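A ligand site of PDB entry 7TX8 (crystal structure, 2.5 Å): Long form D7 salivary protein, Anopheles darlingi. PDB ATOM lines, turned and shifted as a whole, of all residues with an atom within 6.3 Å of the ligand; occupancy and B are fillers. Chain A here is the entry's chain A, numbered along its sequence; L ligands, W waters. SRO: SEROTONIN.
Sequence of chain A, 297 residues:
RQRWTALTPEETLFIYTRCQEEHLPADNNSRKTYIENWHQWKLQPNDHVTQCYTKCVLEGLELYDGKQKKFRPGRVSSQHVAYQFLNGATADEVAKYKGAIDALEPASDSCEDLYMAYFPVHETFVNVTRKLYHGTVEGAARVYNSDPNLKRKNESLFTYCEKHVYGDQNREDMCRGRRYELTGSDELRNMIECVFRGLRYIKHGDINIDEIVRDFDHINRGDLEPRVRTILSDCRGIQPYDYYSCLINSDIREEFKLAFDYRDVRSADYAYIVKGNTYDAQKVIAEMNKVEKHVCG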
ATOM      1  N   PHE A 158       3.339 -27.626  -8.610  1.00  0.00           N
ATOM      2  CA  PHE A 158       2.137 -28.254  -8.105  1.00  0.00           C
ATOM      3  C   PHE A 158       2.045 -29.698  -8.562  1.00  0.00           C
ATOM      4  O   PHE A 158       1.744 -30.586  -7.763  1.00  0.00           O
ATOM      5  CB  PHE A 158       0.894 -27.471  -8.530  1.00  0.00           C
ATOM      6  CG  PHE A 158       0.648 -26.225  -7.724  1.00  0.00           C
ATOM      7  CD1 PHE A 158       1.360 -25.037  -8.001  1.00  0.00           C
ATOM      8  CD2 PHE A 158      -0.286 -26.218  -6.672  1.00  0.00           C
ATOM      9  CE1 PHE A 158       1.154 -23.827  -7.258  1.00  0.00           C
ATOM     10  CE2 PHE A 158      -0.535 -25.047  -5.898  1.00  0.00           C
ATOM     11  CZ  PHE A 158       0.187 -23.822  -6.199  1.00  0.00           C
ATOM     12  N   GLU A 162       2.178 -32.984  -6.316  1.00  0.00           N
ATOM     13  CA  GLU A 162       1.115 -33.978  -6.417  1.00  0.00           C
ATOM     14  C   GLU A 162       1.709 -35.362  -6.579  1.00  0.00           C
ATOM     15  O   GLU A 162       1.303 -36.308  -5.892  1.00  0.00           O
ATOM     16  CB  GLU A 162       0.172 -33.685  -7.594  1.00  0.00           C
ATOM     17  CG  GLU A 162      -0.851 -32.603  -7.340  1.00  0.00           C
ATOM     18  CD  GLU A 162      -1.563 -32.197  -8.614  1.00  0.00           C
ATOM     19  OE1 GLU A 162      -0.907 -32.211  -9.675  1.00  0.00           O
ATOM     20  OE2 GLU A 162      -2.761 -31.878  -8.573  1.00  0.00           O
ATOM     21  N   TYR A 166       0.451 -37.623  -3.493  1.00  0.00           N
ATOM     22  CA  TYR A 166      -0.683 -38.476  -3.816  1.00  0.00           C
ATOM     23  C   TYR A 166      -0.288 -39.733  -4.591  1.00  0.00           C
ATOM     24  O   TYR A 166      -0.977 -40.768  -4.499  1.00  0.00           O
ATOM     25  CB  TYR A 166      -1.703 -37.698  -4.638  1.00  0.00           C
ATOM     26  CG  TYR A 166      -2.445 -36.590  -3.922  1.00  0.00           C
ATOM     27  CD1 TYR A 166      -1.951 -35.283  -3.906  1.00  0.00           C
ATOM     28  CD2 TYR A 166      -3.672 -36.831  -3.309  1.00  0.00           C
ATOM     29  CE1 TYR A 166      -2.653 -34.265  -3.289  1.00  0.00           C
ATOM     30  CE2 TYR A 166      -4.377 -35.824  -2.691  1.00  0.00           C
ATOM     31  CZ  TYR A 166      -3.878 -34.538  -2.672  1.00  0.00           C
ATOM     32  OH  TYR A 166      -4.595 -33.537  -2.044  1.00  0.00           O
ATOM     33  N   ASP A 173      -9.612 -37.369  -4.122  1.00  0.00           N
ATOM     34  CA  ASP A 173      -9.212 -36.318  -3.197  1.00  0.00           C
ATOM     35  C   ASP A 173      -8.268 -35.314  -3.872  1.00  0.00           C
ATOM     36  O   ASP A 173      -8.349 -34.113  -3.593  1.00  0.00           O
ATOM     37  CB  ASP A 173      -8.575 -36.925  -1.947  1.00  0.00           C
ATOM     38  CG  ASP A 173      -8.232 -35.879  -0.885  1.00  0.00           C
ATOM     39  OD1 ASP A 173      -9.131 -35.133  -0.475  1.00  0.00           O
ATOM     40  OD2 ASP A 173      -7.063 -35.807  -0.436  1.00  0.00           O
ATOM     41  N   MET A 174      -7.380 -35.770  -4.758  1.00  0.00           N
ATOM     42  CA  MET A 174      -6.481 -34.826  -5.429  1.00  0.00           C
ATOM     43  C   MET A 174      -7.265 -33.932  -6.388  1.00  0.00           C
ATOM     44  O   MET A 174      -6.938 -32.756  -6.561  1.00  0.00           O
ATOM     45  CB  MET A 174      -5.376 -35.580  -6.177  1.00  0.00           C
ATOM     46  CG  MET A 174      -4.206 -34.712  -6.629  1.00  0.00           C
ATOM     47  SD  MET A 174      -2.898 -35.589  -7.530  1.00  0.00           S
ATOM     48  CE  MET A 174      -3.574 -35.774  -9.193  1.00  0.00           C
ATOM     49  N   CYS A 175      -8.304 -34.492  -6.997  1.00  0.00           N
ATOM     50  CA  CYS A 175      -9.131 -33.717  -7.906  1.00  0.00           C
ATOM     51  C   CYS A 175      -9.871 -32.627  -7.148  1.00  0.00           C
ATOM     52  O   CYS A 175      -9.905 -31.469  -7.567  1.00  0.00           O
ATOM     53  CB  CYS A 175     -10.116 -34.631  -8.625  1.00  0.00           C
ATOM     54  SG  CYS A 175     -11.489 -33.702  -9.388  1.00  0.00           S
ATOM     55  N   ARG A 176     -10.447 -32.995  -6.001  1.00  0.00           N
ATOM     56  CA  ARG A 176     -11.142 -32.005  -5.209  1.00  0.00           C
ATOM     57  C   ARG A 176     -10.161 -30.975  -4.694  1.00  0.00           C
ATOM     58  O   ARG A 176     -10.461 -29.769  -4.704  1.00  0.00           O
ATOM     59  CB  ARG A 176     -11.905 -32.689  -4.051  1.00  0.00           C
ATOM     60  CG  ARG A 176     -13.109 -33.507  -4.514  1.00  0.00           C
ATOM     61  CD  ARG A 176     -13.750 -34.308  -3.405  1.00  0.00           C
ATOM     62  NE  ARG A 176     -14.266 -33.459  -2.334  1.00  0.00           N
ATOM     63  CZ  ARG A 176     -14.043 -33.654  -1.046  1.00  0.00           C
ATOM     64  NH1 ARG A 176     -13.333 -34.693  -0.622  1.00  0.00           N
ATOM     65  NH2 ARG A 176     -14.515 -32.782  -0.175  1.00  0.00           N
ATOM     66  N   GLY A 177      -8.967 -31.399  -4.301  1.00  0.00           N
ATOM     67  CA  GLY A 177      -7.963 -30.460  -3.825  1.00  0.00           C
ATOM     68  C   GLY A 177      -7.523 -29.485  -4.896  1.00  0.00           C
ATOM     69  O   GLY A 177      -7.317 -28.292  -4.626  1.00  0.00           O
ATOM     70  N   ARG A 178      -7.360 -29.964  -6.124  1.00  0.00           N
ATOM     71  CA  ARG A 178      -6.970 -29.082  -7.219  1.00  0.00           C
ATOM     72  C   ARG A 178      -8.085 -28.129  -7.602  1.00  0.00           C
ATOM     73  O   ARG A 178      -7.819 -27.092  -8.219  1.00  0.00           O
ATOM     74  CB  ARG A 178      -6.520 -29.916  -8.418  1.00  0.00           C
ATOM     75  CG  ARG A 178      -6.272 -29.140  -9.683  1.00  0.00           C
ATOM     76  CD  ARG A 178      -5.597 -30.043 -10.707  1.00  0.00           C
ATOM     77  NE  ARG A 178      -4.170 -30.211 -10.406  1.00  0.00           N
ATOM     78  CZ  ARG A 178      -3.235 -29.355 -10.803  1.00  0.00           C
ATOM     79  NH1 ARG A 178      -3.549 -28.267 -11.476  1.00  0.00           N
ATOM     80  NH2 ARG A 178      -1.961 -29.638 -10.581  1.00  0.00           N
ATOM     81  N   ARG A 179      -9.334 -28.452  -7.274  1.00  0.00           N
ATOM     82  CA  ARG A 179     -10.434 -27.500  -7.395  1.00  0.00           C
ATOM     83  C   ARG A 179     -10.589 -26.590  -6.182  1.00  0.00           C
ATOM     84  O   ARG A 179     -11.610 -25.913  -6.056  1.00  0.00           O
ATOM     85  CB  ARG A 179     -11.734 -28.245  -7.650  1.00  0.00           C
ATOM     86  CG  ARG A 179     -11.731 -29.138  -8.845  1.00  0.00           C
ATOM     87  CD  ARG A 179     -13.007 -29.979  -8.837  1.00  0.00           C
ATOM     88  NE  ARG A 179     -13.120 -30.764 -10.061  1.00  0.00           N
ATOM     89  CZ  ARG A 179     -14.096 -31.629 -10.331  1.00  0.00           C
ATOM     90  NH1 ARG A 179     -15.069 -31.867  -9.468  1.00  0.00           N
ATOM     91  NH2 ARG A 179     -14.095 -32.251 -11.505  1.00  0.00           N
ATOM     92  N   TYR A 180      -9.602 -26.579  -5.276  1.00  0.00           N
ATOM     93  CA  TYR A 180      -9.588 -25.673  -4.122  1.00  0.00           C
ATOM     94  C   TYR A 180     -10.600 -26.077  -3.032  1.00  0.00           C
ATOM     95  O   TYR A 180     -11.124 -25.228  -2.313  1.00  0.00           O
ATOM     96  CB  TYR A 180      -9.822 -24.221  -4.546  1.00  0.00           C
ATOM     97  CG  TYR A 180      -8.636 -23.620  -5.271  1.00  0.00           C
ATOM     98  CD1 TYR A 180      -7.519 -23.131  -4.568  1.00  0.00           C
ATOM     99  CD2 TYR A 180      -8.623 -23.521  -6.662  1.00  0.00           C
ATOM    100  CE1 TYR A 180      -6.431 -22.572  -5.225  1.00  0.00           C
ATOM    101  CE2 TYR A 180      -7.547 -22.969  -7.320  1.00  0.00           C
ATOM    102  CZ  TYR A 180      -6.451 -22.516  -6.604  1.00  0.00           C
ATOM    103  OH  TYR A 180      -5.375 -21.964  -7.261  1.00  0.00           O
ATOM    104  N   GLU A 181     -10.860 -27.375  -2.891  1.00  0.00           N
ATOM    105  CA  GLU A 181     -11.666 -27.869  -1.797  1.00  0.00           C
ATOM    106  C   GLU A 181     -10.801 -28.025  -0.549  1.00  0.00           C
ATOM    107  O   GLU A 181      -9.663 -28.488  -0.629  1.00  0.00           O
ATOM    108  CB  GLU A 181     -12.302 -29.213  -2.133  1.00  0.00           C
ATOM    109  CG  GLU A 181     -13.108 -29.273  -3.434  1.00  0.00           C
ATOM    110  CD  GLU A 181     -14.238 -28.257  -3.503  1.00  0.00           C
ATOM    111  OE1 GLU A 181     -14.556 -27.633  -2.464  1.00  0.00           O
ATOM    112  OE2 GLU A 181     -14.794 -28.090  -4.610  1.00  0.00           O
ATOM    113  N   LEU A 188      -3.937 -33.887   1.418  1.00  0.00           N
ATOM    114  CA  LEU A 188      -4.033 -32.471   1.078  1.00  0.00           C
ATOM    115  C   LEU A 188      -3.198 -31.585   2.011  1.00  0.00           C
ATOM    116  O   LEU A 188      -2.665 -30.563   1.587  1.00  0.00           O
ATOM    117  CB  LEU A 188      -5.499 -32.029   1.087  1.00  0.00           C
ATOM    118  CG  LEU A 188      -5.768 -30.574   0.710  1.00  0.00           C
ATOM    119  CD1 LEU A 188      -5.311 -30.319  -0.746  1.00  0.00           C
ATOM    120  CD2 LEU A 188      -7.227 -30.198   0.918  1.00  0.00           C
ATOM    121  N   MET A 191       0.249 -31.910   0.862  1.00  0.00           N
ATOM    122  CA  MET A 191       0.351 -31.234  -0.413  1.00  0.00           C
ATOM    123  C   MET A 191       0.539 -29.742  -0.196  1.00  0.00           C
ATOM    124  O   MET A 191       1.411 -29.117  -0.805  1.00  0.00           O
ATOM    125  CB  MET A 191      -0.883 -31.532  -1.256  1.00  0.00           C
ATOM    126  CG  MET A 191      -1.014 -30.707  -2.523  1.00  0.00           C
ATOM    127  SD  MET A 191       0.138 -31.291  -3.790  1.00  0.00           S
ATOM    128  CE  MET A 191      -0.318 -30.265  -5.173  1.00  0.00           C
ATOM    129  N   ILE A 192      -0.259 -29.163   0.693  1.00  0.00           N
ATOM    130  CA  ILE A 192      -0.147 -27.738   0.891  1.00  0.00           C
ATOM    131  C   ILE A 192       1.189 -27.388   1.544  1.00  0.00           C
ATOM    132  O   ILE A 192       1.803 -26.377   1.218  1.00  0.00           O
ATOM    133  CB  ILE A 192      -1.351 -27.214   1.686  1.00  0.00           C
ATOM    134  CG1 ILE A 192      -2.626 -27.379   0.846  1.00  0.00           C
ATOM    135  CG2 ILE A 192      -1.188 -25.778   2.028  1.00  0.00           C
ATOM    136  CD1 ILE A 192      -2.577 -26.709  -0.533  1.00  0.00           C
ATOM    137  N   VAL A 195       3.784 -27.428  -1.209  1.00  0.00           N
ATOM    138  CA  VAL A 195       3.642 -26.267  -2.100  1.00  0.00           C
ATOM    139  C   VAL A 195       4.145 -25.006  -1.432  1.00  0.00           C
ATOM    140  O   VAL A 195       4.800 -24.166  -2.060  1.00  0.00           O
ATOM    141  CB  VAL A 195       2.167 -26.100  -2.546  1.00  0.00           C
ATOM    142  CG1 VAL A 195       1.963 -24.775  -3.267  1.00  0.00           C
ATOM    143  CG2 VAL A 195       1.741 -27.215  -3.446  1.00  0.00           C
ATOM    144  N   TYR A 244      -3.461 -21.552   4.448  1.00  0.00           N
ATOM    145  CA  TYR A 244      -4.198 -21.857   3.238  1.00  0.00           C
ATOM    146  C   TYR A 244      -5.704 -21.725   3.468  1.00  0.00           C
ATOM    147  O   TYR A 244      -6.387 -21.010   2.738  1.00  0.00           O
ATOM    148  CB  TYR A 244      -3.795 -23.264   2.772  1.00  0.00           C
ATOM    149  CG  TYR A 244      -4.417 -23.739   1.467  1.00  0.00           C
ATOM    150  CD1 TYR A 244      -4.097 -23.118   0.264  1.00  0.00           C
ATOM    151  CD2 TYR A 244      -5.302 -24.820   1.449  1.00  0.00           C
ATOM    152  CE1 TYR A 244      -4.660 -23.556  -0.929  1.00  0.00           C
ATOM    153  CE2 TYR A 244      -5.866 -25.257   0.265  1.00  0.00           C
ATOM    154  CZ  TYR A 244      -5.537 -24.636  -0.917  1.00  0.00           C
ATOM    155  OH  TYR A 244      -6.119 -25.097  -2.069  1.00  0.00           O
ATOM    156  N   LYS A 257      -7.229 -17.469  -5.445  1.00  0.00           N
ATOM    157  CA  LYS A 257      -7.101 -18.510  -6.464  1.00  0.00           C
ATOM    158  C   LYS A 257      -6.421 -17.947  -7.696  1.00  0.00           C
ATOM    159  O   LYS A 257      -5.543 -18.591  -8.290  1.00  0.00           O
ATOM    160  CB  LYS A 257      -8.470 -19.064  -6.836  1.00  0.00           C
ATOM    161  CG  LYS A 257      -9.274 -19.669  -5.710  1.00  0.00           C
ATOM    162  CD  LYS A 257     -10.653 -20.179  -6.198  1.00  0.00           C
ATOM    163  CE  LYS A 257     -11.492 -20.647  -5.018  1.00  0.00           C
ATOM    164  NZ  LYS A 257     -12.817 -21.204  -5.427  1.00  0.00           N
ATOM    165  N   PHE A 260      -2.719 -17.762  -6.744  1.00  0.00           N
ATOM    166  CA  PHE A 260      -2.140 -19.097  -6.630  1.00  0.00           C
ATOM    167  C   PHE A 260      -1.908 -19.699  -8.011  1.00  0.00           C
ATOM    168  O   PHE A 260      -0.824 -20.249  -8.267  1.00  0.00           O
ATOM    169  CB  PHE A 260      -3.061 -19.980  -5.805  1.00  0.00           C
ATOM    170  CG  PHE A 260      -2.336 -20.926  -4.885  1.00  0.00           C
ATOM    171  CD1 PHE A 260      -1.259 -20.495  -4.128  1.00  0.00           C
ATOM    172  CD2 PHE A 260      -2.761 -22.225  -4.737  1.00  0.00           C
ATOM    173  CE1 PHE A 260      -0.565 -21.364  -3.239  1.00  0.00           C
ATOM    174  CE2 PHE A 260      -2.087 -23.090  -3.849  1.00  0.00           C
ATOM    175  CZ  PHE A 260      -0.985 -22.645  -3.102  1.00  0.00           C
ATOM    176  N   ASP A 261      -2.902 -19.605  -8.909  1.00  0.00           N
ATOM    177  CA  ASP A 261      -2.803 -20.183 -10.251  1.00  0.00           C
ATOM    178  C   ASP A 261      -1.730 -19.491 -11.075  1.00  0.00           C
ATOM    179  O   ASP A 261      -0.936 -20.145 -11.775  1.00  0.00           O
ATOM    180  CB  ASP A 261      -4.147 -20.104 -10.982  1.00  0.00           C
ATOM    181  CG  ASP A 261      -5.130 -21.218 -10.590  1.00  0.00           C
ATOM    182  OD1 ASP A 261      -4.746 -22.151  -9.848  1.00  0.00           O
ATOM    183  OD2 ASP A 261      -6.297 -21.145 -11.035  1.00  0.00           O
ATOM    184  N   ASP A 264       1.449 -20.838  -9.836  1.00  0.00           N
ATOM    185  CA  ASP A 264       1.685 -22.177 -10.341  1.00  0.00           C
ATOM    186  C   ASP A 264       2.312 -22.090 -11.727  1.00  0.00           C
ATOM    187  O   ASP A 264       3.351 -22.715 -12.019  1.00  0.00           O
ATOM    188  CB  ASP A 264       0.356 -22.947 -10.364  1.00  0.00           C
ATOM    189  CG  ASP A 264       0.477 -24.396 -10.896  1.00  0.00           C
ATOM    190  OD1 ASP A 264       1.554 -24.838 -11.356  1.00  0.00           O
ATOM    191  OD2 ASP A 264      -0.555 -25.107 -10.864  1.00  0.00           O
ATOM    192  N   MET A 288      -4.645 -24.091 -16.469  1.00  0.00           N
ATOM    193  CA  MET A 288      -5.156 -24.780 -15.272  1.00  0.00           C
ATOM    194  C   MET A 288      -6.300 -25.735 -15.615  1.00  0.00           C
ATOM    195  O   MET A 288      -6.407 -26.801 -15.015  1.00  0.00           O
ATOM    196  CB  MET A 288      -5.647 -23.784 -14.214  1.00  0.00           C
ATOM    197  CG  MET A 288      -4.563 -22.908 -13.655  1.00  0.00           C
ATOM    198  SD  MET A 288      -3.246 -23.841 -12.856  1.00  0.00           S
ATOM    199  CE  MET A 288      -2.238 -24.299 -14.247  1.00  0.00           C
ATOM    200  N   VAL A 291      -5.004 -29.000 -17.159  1.00  0.00           N
ATOM    201  CA  VAL A 291      -4.489 -29.918 -16.136  1.00  0.00           C
ATOM    202  C   VAL A 291      -5.618 -30.479 -15.270  1.00  0.00           C
ATOM    203  O   VAL A 291      -5.663 -31.681 -14.983  1.00  0.00           O
ATOM    204  CB  VAL A 291      -3.390 -29.227 -15.305  1.00  0.00           C
ATOM    205  CG1 VAL A 291      -3.930 -27.976 -14.640  1.00  0.00           C
ATOM    206  CG2 VAL A 291      -2.875 -30.185 -14.268  1.00  0.00           C
HETATM  207  OH  SRO L   1      -3.595 -31.294  -5.903  1.00  0.00           O
HETATM  208  CZ3 SRO L   1      -3.786 -30.000  -5.551  1.00  0.00           C
HETATM  209  CH2 SRO L   1      -4.237 -29.795  -4.234  1.00  0.00           C
HETATM  210  CZ2 SRO L   1      -4.455 -28.524  -3.760  1.00  0.00           C
HETATM  211  CE2 SRO L   1      -4.270 -27.460  -4.637  1.00  0.00           C
HETATM  212  NE1 SRO L   1      -4.437 -26.122  -4.430  1.00  0.00           N
HETATM  213  CD1 SRO L   1      -4.152 -25.458  -5.589  1.00  0.00           C
HETATM  214  CG  SRO L   1      -3.754 -26.331  -6.556  1.00  0.00           C
HETATM  215  CD2 SRO L   1      -3.834 -27.641  -5.958  1.00  0.00           C
HETATM  216  CE3 SRO L   1      -3.585 -28.949  -6.415  1.00  0.00           C
HETATM  217  CB  SRO L   1      -3.368 -26.003  -7.965  1.00  0.00           C
HETATM  218  CA  SRO L   1      -3.788 -24.601  -8.397  1.00  0.00           C
HETATM  219  NZ  SRO L   1      -3.496 -24.375  -9.822  1.00  0.00           N
HETATM  220  O   HOH W   1      -6.161 -25.843 -10.472  1.00  0.00           O
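The side-chain carboxylate (OD1) of Asp 261 is in salt-bridge range of a nitrogen (NZ) of the ligand (2.6 Å).
An oxygen (OH) of the ligand sits at hydrogen-bond distance from the side-chain carboxylate of Glu 162, 2.9 Å away.
The side-chain hydroxyl (OH) of Tyr 244 is in hydrogen-bond range of a nitrogen (NE1) of the ligand (3.1 Å).
A nitrogen (NZ) of the ligand lies within hydrogen-bond range of the side-chain sulfur (SD) of Met 288, at 3.1 Å.
NZ of the ligand is in salt-bridge range of OD2 of Asp 264 (3.2 Å).
The side-chain carboxylate (OD1) of Asp 261 lies within hydrogen-bond range of the side-chain hydroxyl (OH) of Tyr 180 (2.7 Å).
The side-chain carboxylate (OE2) of Glu 162 is in salt-bridge range of the guanidinium group (NE) of Arg 178 (2.9 Å).
The side-chain sulfur of Met 191 sits at hydrogen-bond distance from the backbone NH of Glu 162.
Water W1 bridges O of Arg 178 and NZ of the ligand.
CD2 of Phe 158 touches CB of the ligand (3.3 Å).
CG of Met 174 touches OH of the ligand, 3.5 Å away.
Gly 177 touches the ligand.
Arg 178 touches the ligand (CA to CE3, 3.5 Å).
Tyr 180 touches the ligand (OH to CA, 3.3 Å).
Leu 188 touches the ligand.
CE of Met 191 touches CZ3 of the ligand, 3.5 Å away.
Phe 260 touches the ligand.
Of the 23 residues printed, 13 come within 4 Å of the ligand.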
